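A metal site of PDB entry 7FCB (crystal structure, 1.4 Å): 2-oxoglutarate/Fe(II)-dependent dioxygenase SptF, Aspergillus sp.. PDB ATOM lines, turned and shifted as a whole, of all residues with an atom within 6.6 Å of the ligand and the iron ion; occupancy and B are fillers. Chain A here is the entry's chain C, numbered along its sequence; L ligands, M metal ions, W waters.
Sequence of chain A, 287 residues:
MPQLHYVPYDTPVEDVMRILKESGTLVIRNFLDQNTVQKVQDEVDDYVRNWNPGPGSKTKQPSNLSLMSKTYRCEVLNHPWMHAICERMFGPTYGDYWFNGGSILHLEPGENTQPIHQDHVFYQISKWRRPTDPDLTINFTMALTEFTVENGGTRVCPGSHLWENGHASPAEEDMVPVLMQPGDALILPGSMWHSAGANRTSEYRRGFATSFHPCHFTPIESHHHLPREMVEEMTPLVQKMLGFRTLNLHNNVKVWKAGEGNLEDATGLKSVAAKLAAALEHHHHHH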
ATOM      1  N   THR A  59      17.895 -15.180  25.750  1.00  0.00           N
ATOM      2  CA  THR A  59      18.119 -16.217  24.754  1.00  0.00           C
ATOM      3  C   THR A  59      17.091 -17.315  24.986  1.00  0.00           C
ATOM      4  O   THR A  59      16.922 -17.770  26.119  1.00  0.00           O
ATOM      5  CB  THR A  59      19.535 -16.796  24.857  1.00  0.00           C
ATOM      6  OG1 THR A  59      20.483 -15.789  24.480  1.00  0.00           O
ATOM      7  CG2 THR A  59      19.700 -18.003  23.929  1.00  0.00           C
ATOM      8  N   GLN A  61      16.221 -21.150  23.531  1.00  0.00           N
ATOM      9  CA  GLN A  61      16.631 -22.294  22.707  1.00  0.00           C
ATOM     10  C   GLN A  61      15.769 -23.518  22.961  1.00  0.00           C
ATOM     11  O   GLN A  61      16.262 -24.565  23.388  1.00  0.00           O
ATOM     12  CB  GLN A  61      18.106 -22.608  22.922  1.00  0.00           C
ATOM     13  CG  GLN A  61      19.057 -21.520  22.441  1.00  0.00           C
ATOM     14  CD  GLN A  61      20.451 -22.038  22.190  1.00  0.00           C
ATOM     15  OE1 GLN A  61      20.708 -23.245  22.272  1.00  0.00           O
ATOM     16  NE2 GLN A  61      21.378 -21.124  21.896  1.00  0.00           N
ATOM     17  N   SER A 103      17.693 -26.955  17.884  1.00  0.00           N
ATOM     18  CA  SER A 103      16.830 -26.032  18.598  1.00  0.00           C
ATOM     19  C   SER A 103      16.640 -24.747  17.827  1.00  0.00           C
ATOM     20  O   SER A 103      17.356 -24.428  16.877  1.00  0.00           O
ATOM     21  CB  SER A 103      17.405 -25.708  19.967  1.00  0.00           C
ATOM     22  OG  SER A 103      18.509 -24.851  19.841  1.00  0.00           O
ATOM     23  N   LEU A 105      17.160 -20.867  17.754  1.00  0.00           N
ATOM     24  CA  LEU A 105      18.253 -20.018  18.220  1.00  0.00           C
ATOM     25  C   LEU A 105      17.743 -18.575  18.201  1.00  0.00           C
ATOM     26  O   LEU A 105      17.891 -17.863  17.212  1.00  0.00           O
ATOM     27  CB  LEU A 105      19.464 -20.188  17.304  1.00  0.00           C
ATOM     28  CG  LEU A 105      19.938 -21.630  17.154  1.00  0.00           C
ATOM     29  CD1 LEU A 105      20.943 -21.712  16.015  1.00  0.00           C
ATOM     30  CD2 LEU A 105      20.569 -22.155  18.445  1.00  0.00           C
ATOM     31  N   HIS A 106      17.164 -18.151  19.311  1.00  0.00           N
ATOM     32  CA  HIS A 106      16.396 -16.903  19.366  1.00  0.00           C
ATOM     33  C   HIS A 106      17.086 -15.927  20.315  1.00  0.00           C
ATOM     34  O   HIS A 106      17.269 -16.234  21.495  1.00  0.00           O
ATOM     35  CB  HIS A 106      14.986 -17.228  19.866  1.00  0.00           C
ATOM     36  CG  HIS A 106      14.087 -16.036  19.953  1.00  0.00           C
ATOM     37  ND1 HIS A 106      13.168 -15.725  18.978  1.00  0.00           N
ATOM     38  CD2 HIS A 106      13.977 -15.077  20.907  1.00  0.00           C
ATOM     39  CE1 HIS A 106      12.527 -14.626  19.327  1.00  0.00           C
ATOM     40  NE2 HIS A 106      13.000 -14.219  20.497  1.00  0.00           N
ATOM     41  N   LEU A 107      17.431 -14.748  19.810  1.00  0.00           N
ATOM     42  CA  LEU A 107      18.052 -13.697  20.608  1.00  0.00           C
ATOM     43  C   LEU A 107      17.070 -12.545  20.746  1.00  0.00           C
ATOM     44  O   LEU A 107      16.730 -11.887  19.755  1.00  0.00           O
ATOM     45  CB  LEU A 107      19.318 -13.158  19.943  1.00  0.00           C
ATOM     46  CG  LEU A 107      20.448 -14.145  19.642  1.00  0.00           C
ATOM     47  CD1 LEU A 107      21.659 -13.377  19.151  1.00  0.00           C
ATOM     48  CD2 LEU A 107      20.760 -15.004  20.858  1.00  0.00           C
ATOM     49  N   GLN A 114      27.331 -14.378  23.370  1.00  0.00           N
ATOM     50  CA  GLN A 114      27.444 -15.724  23.889  1.00  0.00           C
ATOM     51  C   GLN A 114      28.918 -16.111  24.007  1.00  0.00           C
ATOM     52  O   GLN A 114      29.731 -15.686  23.182  1.00  0.00           O
ATOM     53  CB  GLN A 114      26.761 -16.687  22.921  1.00  0.00           C
ATOM     54  CG  GLN A 114      26.788 -18.141  23.344  1.00  0.00           C
ATOM     55  CD  GLN A 114      26.151 -19.030  22.320  1.00  0.00           C
ATOM     56  OE1 GLN A 114      26.482 -18.981  21.143  1.00  0.00           O
ATOM     57  NE2 GLN A 114      25.187 -19.821  22.757  1.00  0.00           N
ATOM     58  N   HIS A 117      32.818 -20.856  21.776  1.00  0.00           N
ATOM     59  CA  HIS A 117      32.897 -22.267  22.170  1.00  0.00           C
ATOM     60  C   HIS A 117      33.035 -23.152  20.930  1.00  0.00           C
ATOM     61  O   HIS A 117      32.782 -22.721  19.804  1.00  0.00           O
ATOM     62  CB  HIS A 117      31.633 -22.683  22.936  1.00  0.00           C
ATOM     63  CG  HIS A 117      30.375 -22.550  22.143  1.00  0.00           C
ATOM     64  ND1 HIS A 117      29.719 -21.342  21.969  1.00  0.00           N
ATOM     65  CD2 HIS A 117      29.680 -23.456  21.412  1.00  0.00           C
ATOM     66  CE1 HIS A 117      28.661 -21.523  21.198  1.00  0.00           C
ATOM     67  NE2 HIS A 117      28.612 -22.803  20.856  1.00  0.00           N
ATOM     68  N   GLN A 118      33.446 -24.399  21.172  1.00  0.00           N
ATOM     69  CA  GLN A 118      33.291 -25.474  20.200  1.00  0.00           C
ATOM     70  C   GLN A 118      32.116 -26.333  20.641  1.00  0.00           C
ATOM     71  O   GLN A 118      31.986 -26.654  21.825  1.00  0.00           O
ATOM     72  CB  GLN A 118      34.526 -26.368  20.174  1.00  0.00           C
ATOM     73  CG  GLN A 118      35.810 -25.665  19.744  1.00  0.00           C
ATOM     74  CD  GLN A 118      37.012 -26.572  19.899  1.00  0.00           C
ATOM     75  OE1 GLN A 118      37.333 -26.981  21.023  1.00  0.00           O
ATOM     76  NE2 GLN A 118      37.666 -26.902  18.794  1.00  0.00           N
ATOM     77  N   ASP A 119      31.250 -26.717  19.683  1.00  0.00           N
ATOM     78  CA  ASP A 119      30.093 -27.518  20.078  1.00  0.00           C
ATOM     79  C   ASP A 119      30.475 -28.890  20.612  1.00  0.00           C
ATOM     80  O   ASP A 119      29.700 -29.493  21.349  1.00  0.00           O
ATOM     81  CB  ASP A 119      29.123 -27.695  18.902  1.00  0.00           C
ATOM     82  CG  ASP A 119      28.314 -26.450  18.597  1.00  0.00           C
ATOM     83  OD1 ASP A 119      28.248 -25.524  19.446  1.00  0.00           O
ATOM     84  OD2 ASP A 119      27.747 -26.431  17.480  1.00  0.00           O
ATOM     85  N   ASN A 139      26.668 -29.206  12.712  1.00  0.00           N
ATOM     86  CA  ASN A 139      25.458 -28.418  12.929  1.00  0.00           C
ATOM     87  C   ASN A 139      25.181 -27.590  11.668  1.00  0.00           C
ATOM     88  O   ASN A 139      26.117 -27.139  11.001  1.00  0.00           O
ATOM     89  CB  ASN A 139      25.712 -27.514  14.153  1.00  0.00           C
ATOM     90  CG  ASN A 139      24.723 -26.383  14.279  1.00  0.00           C
ATOM     91  OD1 ASN A 139      24.664 -25.507  13.445  1.00  0.00           O
ATOM     92  ND2 ASN A 139      23.947 -26.399  15.369  1.00  0.00           N
ATOM     93  N   THR A 141      23.065 -24.265  10.906  1.00  0.00           N
ATOM     94  CA  THR A 141      22.379 -23.143  11.560  1.00  0.00           C
ATOM     95  C   THR A 141      21.711 -22.316  10.458  1.00  0.00           C
ATOM     96  O   THR A 141      22.400 -21.641   9.672  1.00  0.00           O
ATOM     97  CB  THR A 141      23.360 -22.339  12.399  1.00  0.00           C
ATOM     98  OG1 THR A 141      23.658 -23.066  13.597  1.00  0.00           O
ATOM     99  CG2 THR A 141      22.777 -20.982  12.818  1.00  0.00           C
ATOM    100  N   PHE A 147      20.468 -12.399   9.625  1.00  0.00           N
ATOM    101  CA  PHE A 147      21.560 -12.373  10.592  1.00  0.00           C
ATOM    102  C   PHE A 147      22.459 -11.209  10.190  1.00  0.00           C
ATOM    103  O   PHE A 147      22.967 -11.175   9.064  1.00  0.00           O
ATOM    104  CB  PHE A 147      22.366 -13.666  10.540  1.00  0.00           C
ATOM    105  CG  PHE A 147      21.820 -14.792  11.400  1.00  0.00           C
ATOM    106  CD1 PHE A 147      20.453 -14.949  11.621  1.00  0.00           C
ATOM    107  CD2 PHE A 147      22.692 -15.715  11.971  1.00  0.00           C
ATOM    108  CE1 PHE A 147      19.986 -16.023  12.392  1.00  0.00           C
ATOM    109  CE2 PHE A 147      22.230 -16.757  12.735  1.00  0.00           C
ATOM    110  CZ  PHE A 147      20.873 -16.913  12.966  1.00  0.00           C
ATOM    111  N   GLY A 152      23.232  -9.732  16.335  1.00  0.00           N
ATOM    112  CA  GLY A 152      23.821 -10.876  17.000  1.00  0.00           C
ATOM    113  C   GLY A 152      24.049 -12.087  16.119  1.00  0.00           C
ATOM    114  O   GLY A 152      24.161 -13.200  16.658  1.00  0.00           O
ATOM    115  N   GLY A 153      24.099 -11.911  14.805  1.00  0.00           N
ATOM    116  CA  GLY A 153      24.426 -13.001  13.909  1.00  0.00           C
ATOM    117  C   GLY A 153      25.643 -13.763  14.388  1.00  0.00           C
ATOM    118  O   GLY A 153      26.602 -13.178  14.918  1.00  0.00           O
ATOM    119  N   THR A 154      25.600 -15.093  14.252  1.00  0.00           N
ATOM    120  CA  THR A 154      26.690 -15.955  14.688  1.00  0.00           C
ATOM    121  C   THR A 154      28.019 -15.466  14.126  1.00  0.00           C
ATOM    122  O   THR A 154      28.107 -14.955  13.012  1.00  0.00           O
ATOM    123  CB  THR A 154      26.437 -17.375  14.152  1.00  0.00           C
ATOM    124  OG1 THR A 154      25.044 -17.683  14.310  1.00  0.00           O
ATOM    125  CG2 THR A 154      27.283 -18.403  14.916  1.00  0.00           C
ATOM    126  N   ARG A 155      29.081 -15.644  14.925  1.00  0.00           N
ATOM    127  CA  ARG A 155      30.435 -15.327  14.508  1.00  0.00           C
ATOM    128  C   ARG A 155      31.280 -16.593  14.568  1.00  0.00           C
ATOM    129  O   ARG A 155      31.064 -17.458  15.426  1.00  0.00           O
ATOM    130  CB  ARG A 155      31.039 -14.272  15.438  1.00  0.00           C
ATOM    131  CG  ARG A 155      30.157 -13.046  15.617  1.00  0.00           C
ATOM    132  CD  ARG A 155      29.275 -13.127  16.878  1.00  0.00           C
ATOM    133  NE  ARG A 155      30.034 -13.595  18.027  1.00  0.00           N
ATOM    134  CZ  ARG A 155      30.932 -12.870  18.672  1.00  0.00           C
ATOM    135  NH1 ARG A 155      31.134 -11.601  18.363  1.00  0.00           N
ATOM    136  NH2 ARG A 155      31.661 -13.437  19.633  1.00  0.00           N
ATOM    137  N   LEU A 186      24.518 -21.586   7.849  1.00  0.00           N
ATOM    138  CA  LEU A 186      25.899 -21.675   8.299  1.00  0.00           C
ATOM    139  C   LEU A 186      26.205 -23.100   8.722  1.00  0.00           C
ATOM    140  O   LEU A 186      25.451 -23.694   9.508  1.00  0.00           O
ATOM    141  CB  LEU A 186      26.079 -20.706   9.472  1.00  0.00           C
ATOM    142  CG  LEU A 186      27.387 -20.727  10.243  1.00  0.00           C
ATOM    143  CD1 LEU A 186      28.566 -20.314   9.360  1.00  0.00           C
ATOM    144  CD2 LEU A 186      27.273 -19.813  11.455  1.00  0.00           C
ATOM    145  N   LEU A 188      28.528 -25.654  10.739  1.00  0.00           N
ATOM    146  CA  LEU A 188      29.379 -25.600  11.930  1.00  0.00           C
ATOM    147  C   LEU A 188      29.782 -27.006  12.329  1.00  0.00           C
ATOM    148  O   LEU A 188      29.079 -27.663  13.108  1.00  0.00           O
ATOM    149  CB  LEU A 188      28.647 -24.933  13.098  1.00  0.00           C
ATOM    150  CG  LEU A 188      28.379 -23.446  12.951  1.00  0.00           C
ATOM    151  CD1 LEU A 188      27.471 -22.999  14.078  1.00  0.00           C
ATOM    152  CD2 LEU A 188      29.694 -22.668  12.958  1.00  0.00           C
ATOM    153  N   MET A 192      34.676 -26.151  15.141  1.00  0.00           N
ATOM    154  CA  MET A 192      34.790 -24.725  14.829  1.00  0.00           C
ATOM    155  C   MET A 192      34.435 -23.885  16.046  1.00  0.00           C
ATOM    156  O   MET A 192      33.379 -24.066  16.652  1.00  0.00           O
ATOM    157  CB  MET A 192      33.850 -24.379  13.668  1.00  0.00           C
ATOM    158  CG  MET A 192      33.697 -22.872  13.416  1.00  0.00           C
ATOM    159  SD  MET A 192      35.250 -21.987  13.171  1.00  0.00           S
ATOM    160  CE  MET A 192      35.977 -22.838  11.785  1.00  0.00           C
ATOM    161  N   HIS A 194      32.988 -20.645  17.687  1.00  0.00           N
ATOM    162  CA  HIS A 194      31.949 -19.732  17.233  1.00  0.00           C
ATOM    163  C   HIS A 194      31.114 -19.279  18.428  1.00  0.00           C
ATOM    164  O   HIS A 194      31.204 -19.828  19.531  1.00  0.00           O
ATOM    165  CB  HIS A 194      31.027 -20.437  16.229  1.00  0.00           C
ATOM    166  CG  HIS A 194      30.272 -21.576  16.837  1.00  0.00           C
ATOM    167  ND1 HIS A 194      30.843 -22.812  17.052  1.00  0.00           N
ATOM    168  CD2 HIS A 194      29.009 -21.648  17.322  1.00  0.00           C
ATOM    169  CE1 HIS A 194      29.954 -23.604  17.627  1.00  0.00           C
ATOM    170  NE2 HIS A 194      28.843 -22.918  17.820  1.00  0.00           N
ATOM    171  N   SER A 195      30.250 -18.293  18.174  1.00  0.00           N
ATOM    172  CA  SER A 195      29.288 -17.898  19.208  1.00  0.00           C
ATOM    173  C   SER A 195      28.250 -16.960  18.606  1.00  0.00           C
ATOM    174  O   SER A 195      28.498 -16.299  17.598  1.00  0.00           O
ATOM    175  CB  SER A 195      29.964 -17.201  20.394  1.00  0.00           C
ATOM    176  OG  SER A 195      29.994 -15.793  20.226  1.00  0.00           O
ATOM    177  N   ALA A 196      27.077 -16.939  19.236  1.00  0.00           N
ATOM    178  CA  ALA A 196      26.110 -15.887  18.952  1.00  0.00           C
ATOM    179  C   ALA A 196      26.668 -14.540  19.417  1.00  0.00           C
ATOM    180  O   ALA A 196      27.413 -14.444  20.396  1.00  0.00           O
ATOM    181  CB  ALA A 196      24.804 -16.186  19.700  1.00  0.00           C
ATOM    182  N   GLY A 197      26.296 -13.484  18.694  1.00  0.00           N
ATOM    183  CA  GLY A 197      26.670 -12.141  19.077  1.00  0.00           C
ATOM    184  C   GLY A 197      25.614 -11.480  19.938  1.00  0.00           C
ATOM    185  O   GLY A 197      24.577 -12.049  20.268  1.00  0.00           O
ATOM    186  N   ARG A 205      16.444 -11.718  16.758  1.00  0.00           N
ATOM    187  CA  ARG A 205      17.159 -12.441  15.716  1.00  0.00           C
ATOM    188  C   ARG A 205      16.922 -13.931  15.937  1.00  0.00           C
ATOM    189  O   ARG A 205      17.208 -14.436  17.034  1.00  0.00           O
ATOM    190  CB  ARG A 205      18.665 -12.155  15.781  1.00  0.00           C
ATOM    191  CG  ARG A 205      19.467 -12.912  14.722  1.00  0.00           C
ATOM    192  CD  ARG A 205      20.687 -13.614  15.316  1.00  0.00           C
ATOM    193  NE  ARG A 205      20.304 -14.829  16.021  1.00  0.00           N
ATOM    194  CZ  ARG A 205      21.172 -15.757  16.421  1.00  0.00           C
ATOM    195  NH1 ARG A 205      22.478 -15.586  16.264  1.00  0.00           N
ATOM    196  NH2 ARG A 205      20.728 -16.886  16.965  1.00  0.00           N
HETATM  197  C1  LIG L   1      24.933 -22.532  20.389  1.00  0.00           C
HETATM  198  C2  LIG L   1      25.336 -21.553  19.321  1.00  0.00           C
HETATM  199  C3  LIG L   1      24.836 -19.667  17.893  1.00  0.00           C
HETATM  200  C4  LIG L   1      23.741 -18.645  17.593  1.00  0.00           C
HETATM  201  O1  LIG L   1      23.937 -22.239  21.054  1.00  0.00           O
HETATM  202  O2  LIG L   1      25.643 -23.540  20.497  1.00  0.00           O
HETATM  203  O3  LIG L   1      26.432 -21.698  18.784  1.00  0.00           O
HETATM  204  O4  LIG L   1      22.660 -18.740  18.208  1.00  0.00           O
HETATM  205  N1  LIG L   1      24.484 -20.595  18.953  1.00  0.00           N
HETATM  206  O5  LIG L   1      24.011 -17.791  16.731  1.00  0.00           O
HETATM  207 FE    FE M   1      27.371 -23.543  19.210  1.00  0.00          FE
HETATM  208  O   HOH W   1      24.422 -25.845  21.366  1.00  0.00           O
HETATM  209  O   HOH W   2      22.060 -24.957  20.057  1.00  0.00           O
HETATM  210  O   HOH W   3      23.716 -23.334  23.751  1.00  0.00           O
HETATM  211  O   HOH W   4      22.041 -18.658  20.987  1.00  0.00           O
HETATM  212  O   HOH W   5      24.413 -22.679  16.229  1.00  0.00           O
HETATM  213  O   HOH W   6      26.076 -24.410  17.717  1.00  0.00           O
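NE2 of Gln 61 lies within hydrogen-bond range of O1 of the ligand (2.9 Å).
The side-chain hydroxyl of Thr 154 is in hydrogen-bond range of an oxygen (O5) of the ligand.
O5 of the ligand is in salt-bridge range of NH1 of Arg 205, 2.7 Å away.
The side-chain amide nitrogen (NE2) of Gln 114 lies within hydrogen-bond range of an oxygen (O1) of the ligand.
N of Leu 107 sits at hydrogen-bond distance from O of Arg 205 (2.8 Å).
The side-chain amide oxygen (OE1) of Gln 114 is in hydrogen-bond range of the backbone NH (N) of Ala 196 (2.9 Å).
The guanidinium group (NH1) of Arg 205 is in hydrogen-bond range of the backbone carbonyl oxygen (O) of Gly 152 (2.9 Å).
The backbone carbonyl oxygen (O) of Met 192 lies within hydrogen-bond range of a ring nitrogen (ND1) of His 194, at 2.9 Å.
OG of Ser 195 is in hydrogen-bond range of O of Gln 114.
O of Leu 105 sits at hydrogen-bond distance from NH2 of Arg 205 (3.0 Å).
Leu 105 touches the ligand (CB to O4, 3.6 Å).
CB of Ala 196 touches C4 of the ligand, 3.4 Å away.
Hydrophobic or aromatic side chains within 4 Å of the ligand: Leu 105, His 117, His 194 and Ala 196.
Nine residues have an atom within 4 Å of the ligand: Gln 61, Leu 105, Gln 114, His 117, Asp 119, Thr 154, His 194, Ala 196 and Arg 205.
Three residues have an atom within 4 Å of the iron ion: His 117, Asp 119 and His 194.
O3 of the ligand binds the iron ion.
The iron ion is bound by NE2 of His 194 (2.1 Å).
The iron ion is bound by an oxygen (O2) of the ligand, at 2.2 Å.
Water W6 is bound to the iron ion, 2.2 Å away.
OD1 of Asp 119 is bound to the iron ion, at 2.2 Å.
NE2 of His 117 binds the iron ion (2.2 Å).
The iron ion has six donor atoms within binding distance.
Water W4 lies within hydrogen-bond range of the side-chain amide nitrogen (NE2) of Gln 61 (2.7 Å) and an oxygen (O4) of the ligand (2.8 Å).
Water W3 bridges an oxygen (O1) of the ligand (2.9 Å) and the side-chain amide oxygen (OE1) of Gln 61 (3.4 Å).
Water W5 bridges the side-chain hydroxyl (OG1) of Thr 141 and a nitrogen (N1) of the ligand.
Water W2 lies within hydrogen-bond range of the side-chain amide oxygen (OE1) of Gln 61 (3.1 Å) and an oxygen (O1) of the ligand (3.5 Å).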
